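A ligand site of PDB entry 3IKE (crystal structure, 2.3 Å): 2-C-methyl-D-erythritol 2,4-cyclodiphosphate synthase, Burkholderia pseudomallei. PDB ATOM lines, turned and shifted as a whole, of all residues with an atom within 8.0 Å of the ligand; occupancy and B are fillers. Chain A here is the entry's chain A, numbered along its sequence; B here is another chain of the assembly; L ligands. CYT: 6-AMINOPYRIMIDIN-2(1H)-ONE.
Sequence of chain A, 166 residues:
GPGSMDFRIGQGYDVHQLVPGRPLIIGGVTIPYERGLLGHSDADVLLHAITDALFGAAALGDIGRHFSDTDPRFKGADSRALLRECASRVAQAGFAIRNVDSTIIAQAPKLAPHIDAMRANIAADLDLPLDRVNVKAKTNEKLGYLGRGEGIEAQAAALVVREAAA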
ATOM      1  N   ILE A 104      -7.536  34.392  16.838  1.00  0.00           N
ATOM      2  CA  ILE A 104      -8.725  34.016  17.578  1.00  0.00           C
ATOM      3  C   ILE A 104      -8.356  32.805  18.436  1.00  0.00           C
ATOM      4  O   ILE A 104      -7.752  31.851  17.950  1.00  0.00           O
ATOM      5  CB  ILE A 104      -9.894  33.575  16.626  1.00  0.00           C
ATOM      6  CG1 ILE A 104     -10.095  34.594  15.500  1.00  0.00           C
ATOM      7  CG2 ILE A 104     -11.223  33.299  17.421  1.00  0.00           C
ATOM      8  CD1 ILE A 104     -10.824  34.041  14.309  1.00  0.00           C
ATOM      9  N   ILE A 105      -8.759  32.833  19.697  1.00  0.00           N
ATOM     10  CA  ILE A 105      -8.601  31.665  20.541  1.00  0.00           C
ATOM     11  C   ILE A 105      -9.972  31.119  20.957  1.00  0.00           C
ATOM     12  O   ILE A 105     -10.772  31.830  21.590  1.00  0.00           O
ATOM     13  CB  ILE A 105      -7.788  31.996  21.795  1.00  0.00           C
ATOM     14  CG1 ILE A 105      -6.592  32.871  21.413  1.00  0.00           C
ATOM     15  CG2 ILE A 105      -7.357  30.693  22.529  1.00  0.00           C
ATOM     16  CD1 ILE A 105      -6.191  33.795  22.548  1.00  0.00           C
ATOM     17  N   ALA A 106     -10.226  29.884  20.590  1.00  0.00           N
ATOM     18  CA  ALA A 106     -11.498  29.230  20.839  1.00  0.00           C
ATOM     19  C   ALA A 106     -11.305  27.731  20.942  1.00  0.00           C
ATOM     20  O   ALA A 106     -10.641  27.127  20.092  1.00  0.00           O
ATOM     21  CB  ALA A 106     -12.488  29.548  19.736  1.00  0.00           C
ATOM     22  N   GLN A 107     -11.915  27.151  21.966  1.00  0.00           N
ATOM     23  CA  GLN A 107     -11.935  25.704  22.148  1.00  0.00           C
ATOM     24  C   GLN A 107     -12.734  25.121  20.975  1.00  0.00           C
ATOM     25  O   GLN A 107     -12.324  24.115  20.389  1.00  0.00           O
ATOM     26  CB  GLN A 107     -12.544  25.354  23.519  1.00  0.00           C
ATOM     27  CG  GLN A 107     -12.397  23.889  23.975  1.00  0.00           C
ATOM     28  CD  GLN A 107     -13.460  22.950  23.387  1.00  0.00           C
ATOM     29  OE1 GLN A 107     -14.651  23.322  23.173  1.00  0.00           O
ATOM     30  NE2 GLN A 107     -13.038  21.717  23.109  1.00  0.00           N
ATOM     31  N   ALA A 108     -13.818  25.804  20.606  1.00  0.00           N
ATOM     32  CA  ALA A 108     -14.755  25.369  19.559  1.00  0.00           C
ATOM     33  C   ALA A 108     -15.584  26.579  19.119  1.00  0.00           C
ATOM     34  O   ALA A 108     -15.661  27.553  19.848  1.00  0.00           O
ATOM     35  CB  ALA A 108     -15.701  24.235  20.081  1.00  0.00           C
ATOM     36  N   PRO A 109     -16.222  26.533  17.930  1.00  0.00           N
ATOM     37  CA  PRO A 109     -16.165  25.455  16.918  1.00  0.00           C
ATOM     38  C   PRO A 109     -14.847  25.496  16.137  1.00  0.00           C
ATOM     39  O   PRO A 109     -13.955  26.316  16.483  1.00  0.00           O
ATOM     40  CB  PRO A 109     -17.382  25.779  16.015  1.00  0.00           C
ATOM     41  CG  PRO A 109     -17.554  27.265  16.148  1.00  0.00           C
ATOM     42  CD  PRO A 109     -17.106  27.642  17.512  1.00  0.00           C
ATOM     43  N   LYS A 110     -14.706  24.592  15.166  1.00  0.00           N
ATOM     44  CA  LYS A 110     -13.584  24.636  14.212  1.00  0.00           C
ATOM     45  C   LYS A 110     -13.723  25.933  13.444  1.00  0.00           C
ATOM     46  O   LYS A 110     -14.786  26.158  12.845  1.00  0.00           O
ATOM     47  CB  LYS A 110     -13.636  23.510  13.150  1.00  0.00           C
ATOM     48  CG  LYS A 110     -13.612  22.099  13.648  1.00  0.00           C
ATOM     49  CD  LYS A 110     -12.212  21.522  13.838  1.00  0.00           C
ATOM     50  CE  LYS A 110     -12.262  20.335  14.892  1.00  0.00           C
ATOM     51  NZ  LYS A 110     -11.193  20.483  15.968  1.00  0.00           N
ATOM     52  N   LEU A 111     -12.656  26.746  13.438  1.00  0.00           N
ATOM     53  CA  LEU A 111     -12.670  28.042  12.764  1.00  0.00           C
ATOM     54  C   LEU A 111     -12.004  28.010  11.391  1.00  0.00           C
ATOM     55  O   LEU A 111     -12.298  28.872  10.548  1.00  0.00           O
ATOM     56  CB  LEU A 111     -12.042  29.137  13.632  1.00  0.00           C
ATOM     57  CG  LEU A 111     -12.620  29.338  15.035  1.00  0.00           C
ATOM     58  CD1 LEU A 111     -11.659  30.202  15.851  1.00  0.00           C
ATOM     59  CD2 LEU A 111     -14.048  29.934  15.039  1.00  0.00           C
ATOM     60  N   ALA A 112     -11.102  27.035  11.167  1.00  0.00           N
ATOM     61  CA  ALA A 112     -10.408  26.926   9.872  1.00  0.00           C
ATOM     62  C   ALA A 112     -11.308  27.072   8.641  1.00  0.00           C
ATOM     63  O   ALA A 112     -10.945  27.782   7.723  1.00  0.00           O
ATOM     64  CB  ALA A 112      -9.544  25.614   9.761  1.00  0.00           C
ATOM     65  N   PRO A 113     -12.491  26.387   8.603  1.00  0.00           N
ATOM     66  CA  PRO A 113     -13.310  26.545   7.359  1.00  0.00           C
ATOM     67  C   PRO A 113     -13.892  27.963   7.081  1.00  0.00           C
ATOM     68  O   PRO A 113     -14.398  28.202   5.972  1.00  0.00           O
ATOM     69  CB  PRO A 113     -14.445  25.509   7.506  1.00  0.00           C
ATOM     70  CG  PRO A 113     -14.150  24.700   8.779  1.00  0.00           C
ATOM     71  CD  PRO A 113     -13.029  25.381   9.542  1.00  0.00           C
ATOM     72  N   HIS A 114     -13.800  28.868   8.047  1.00  0.00           N
ATOM     73  CA  HIS A 114     -14.366  30.224   7.918  1.00  0.00           C
ATOM     74  C   HIS A 114     -13.334  31.319   7.851  1.00  0.00           C
ATOM     75  O   HIS A 114     -13.686  32.481   7.645  1.00  0.00           O
ATOM     76  CB  HIS A 114     -15.321  30.508   9.072  1.00  0.00           C
ATOM     77  CG  HIS A 114     -16.254  29.383   9.332  1.00  0.00           C
ATOM     78  ND1 HIS A 114     -17.364  29.147   8.548  1.00  0.00           N
ATOM     79  CD2 HIS A 114     -16.230  28.398  10.273  1.00  0.00           C
ATOM     80  CE1 HIS A 114     -17.992  28.076   9.002  1.00  0.00           C
ATOM     81  NE2 HIS A 114     -17.322  27.602  10.056  1.00  0.00           N
ATOM     82  N   ILE A 115     -12.066  30.961   8.000  1.00  0.00           N
ATOM     83  CA  ILE A 115     -10.994  31.940   8.147  1.00  0.00           C
ATOM     84  C   ILE A 115     -10.794  32.783   6.899  1.00  0.00           C
ATOM     85  O   ILE A 115     -10.618  34.014   6.989  1.00  0.00           O
ATOM     86  CB  ILE A 115      -9.701  31.242   8.542  1.00  0.00           C
ATOM     87  CG1 ILE A 115      -9.781  30.778   9.990  1.00  0.00           C
ATOM     88  CG2 ILE A 115      -8.523  32.162   8.331  1.00  0.00           C
ATOM     89  CD1 ILE A 115      -9.544  31.820  10.975  1.00  0.00           C
ATOM     90  N   LYS A 136      -5.440  34.300  12.347  1.00  0.00           N
ATOM     91  CA  LYS A 136      -4.936  33.024  12.861  1.00  0.00           C
ATOM     92  C   LYS A 136      -5.903  32.481  13.936  1.00  0.00           C
ATOM     93  O   LYS A 136      -6.655  33.237  14.595  1.00  0.00           O
ATOM     94  CB  LYS A 136      -3.512  33.196  13.424  1.00  0.00           C
ATOM     95  CG  LYS A 136      -2.510  33.844  12.417  1.00  0.00           C
ATOM     96  CD  LYS A 136      -1.045  34.024  12.936  1.00  0.00           C
ATOM     97  CE  LYS A 136      -0.962  34.843  14.232  1.00  0.00           C
ATOM     98  NZ  LYS A 136      -1.596  36.200  14.074  1.00  0.00           N
ATOM     99  N   ALA A 137      -5.896  31.170  14.113  1.00  0.00           N
ATOM    100  CA  ALA A 137      -6.850  30.558  15.017  1.00  0.00           C
ATOM    101  C   ALA A 137      -6.142  29.569  15.912  1.00  0.00           C
ATOM    102  O   ALA A 137      -5.393  28.751  15.427  1.00  0.00           O
ATOM    103  CB  ALA A 137      -7.981  29.905  14.238  1.00  0.00           C
ATOM    104  N   LYS A 138      -6.362  29.684  17.228  1.00  0.00           N
ATOM    105  CA  LYS A 138      -5.711  28.835  18.212  1.00  0.00           C
ATOM    106  C   LYS A 138      -6.764  28.227  19.132  1.00  0.00           C
ATOM    107  O   LYS A 138      -7.799  28.866  19.361  1.00  0.00           O
ATOM    108  CB  LYS A 138      -4.812  29.674  19.121  1.00  0.00           C
ATOM    109  CG  LYS A 138      -3.993  30.664  18.410  1.00  0.00           C
ATOM    110  CD  LYS A 138      -2.507  30.311  18.261  1.00  0.00           C
ATOM    111  CE  LYS A 138      -2.189  28.865  17.965  1.00  0.00           C
ATOM    112  NZ  LYS A 138      -1.484  28.255  19.141  1.00  0.00           N
ATOM    113  N   THR A 139      -6.476  27.049  19.679  1.00  0.00           N
ATOM    114  CA  THR A 139      -7.200  26.610  20.868  1.00  0.00           C
ATOM    115  C   THR A 139      -6.363  27.178  22.014  1.00  0.00           C
ATOM    116  O   THR A 139      -5.217  27.641  21.779  1.00  0.00           O
ATOM    117  CB  THR A 139      -7.260  25.063  21.011  1.00  0.00           C
ATOM    118  OG1 THR A 139      -5.976  24.584  21.440  1.00  0.00           O
ATOM    119  CG2 THR A 139      -7.657  24.359  19.676  1.00  0.00           C
ATOM    120  N   ASN A 140      -6.884  27.109  23.244  1.00  0.00           N
ATOM    121  CA  ASN A 140      -6.054  27.457  24.415  1.00  0.00           C
ATOM    122  C   ASN A 140      -5.381  26.209  25.054  1.00  0.00           C
ATOM    123  O   ASN A 140      -5.063  26.200  26.265  1.00  0.00           O
ATOM    124  CB  ASN A 140      -6.851  28.268  25.467  1.00  0.00           C
ATOM    125  CG  ASN A 140      -5.985  29.338  26.140  1.00  0.00           C
ATOM    126  OD1 ASN A 140      -5.212  30.021  25.468  1.00  0.00           O
ATOM    127  ND2 ASN A 140      -6.124  29.524  27.467  1.00  0.00           N
ATOM    128  N   ILE A 152     -14.620  33.442  23.970  1.00  0.00           N
ATOM    129  CA  ILE A 152     -13.695  33.451  22.859  1.00  0.00           C
ATOM    130  C   ILE A 152     -12.934  34.765  22.890  1.00  0.00           C
ATOM    131  O   ILE A 152     -13.520  35.829  23.116  1.00  0.00           O
ATOM    132  CB  ILE A 152     -14.405  33.241  21.505  1.00  0.00           C
ATOM    133  CG1 ILE A 152     -15.026  31.848  21.441  1.00  0.00           C
ATOM    134  CG2 ILE A 152     -13.421  33.543  20.301  1.00  0.00           C
ATOM    135  CD1 ILE A 152     -15.841  31.555  20.153  1.00  0.00           C
ATOM    136  N   ASP B  62      -1.155  30.640   9.411  1.00  0.00           N
ATOM    137  CA  ASP B  62      -0.626  30.279  10.712  1.00  0.00           C
ATOM    138  C   ASP B  62       0.013  28.900  10.742  1.00  0.00           C
ATOM    139  O   ASP B  62       0.056  28.175   9.737  1.00  0.00           O
ATOM    140  CB  ASP B  62      -1.718  30.358  11.782  1.00  0.00           C
ATOM    141  CG  ASP B  62      -2.857  29.377  11.560  1.00  0.00           C
ATOM    142  OD1 ASP B  62      -2.679  28.369  10.821  1.00  0.00           O
ATOM    143  OD2 ASP B  62      -3.948  29.623  12.123  1.00  0.00           O
ATOM    144  N   GLY B  64      -1.047  26.133  12.170  1.00  0.00           N
ATOM    145  CA  GLY B  64      -1.987  25.036  11.840  1.00  0.00           C
ATOM    146  C   GLY B  64      -2.201  24.765  10.346  1.00  0.00           C
ATOM    147  O   GLY B  64      -2.426  23.623   9.926  1.00  0.00           O
HETATM  148  N3  CYT L   1     -10.539  26.164  15.291  1.00  0.00           N
HETATM  149  C4  CYT L   1     -10.374  26.467  16.587  1.00  0.00           C
HETATM  150  N1  CYT L   1      -8.190  25.933  15.100  1.00  0.00           N
HETATM  151  C2  CYT L   1      -9.453  25.890  14.507  1.00  0.00           C
HETATM  152  O2  CYT L   1      -9.534  25.604  13.297  1.00  0.00           O
HETATM  153  N4  CYT L   1     -11.450  26.739  17.334  1.00  0.00           N
HETATM  154  C5  CYT L   1      -9.097  26.506  17.195  1.00  0.00           C
HETATM  155  C6  CYT L   1      -8.031  26.232  16.419  1.00  0.00           C
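Merely in contact with the ligand: Lys 138, Lys 110, Thr 139 and Ala 137. Hydrophobic or aromatic side chains within 4 Å of the ligand: Ala 106, Leu 111 and Ala 112. Within 4 Å of the ligand: Ala 106, Pro 109, Lys 110, Leu 111, Ala 112, Ala 137, Lys 138 and Thr 139.
O of Pro 109 sits at hydrogen-bond distance from N4 of the ligand (2.7 Å). The backbone NH (N) of Leu 111 is in hydrogen-bond range of an oxygen (O2) of the ligand (3.3 Å). O2 of the ligand lies within hydrogen-bond range of N of Ala 112 (3.0 Å). A nitrogen (N4) of the ligand is in hydrogen-bond range of the backbone carbonyl oxygen of Ala 106 (2.9 Å).
N of Lys 138 sits at hydrogen-bond distance from O of Ile 104 (2.7 Å). OD2 of Asp 62 of chain B lies within hydrogen-bond range of N of Ala 137 (3.2 Å). The backbone carbonyl oxygen (O) of Lys 138 is in hydrogen-bond range of the backbone NH (N) of Ala 106 (2.9 Å).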
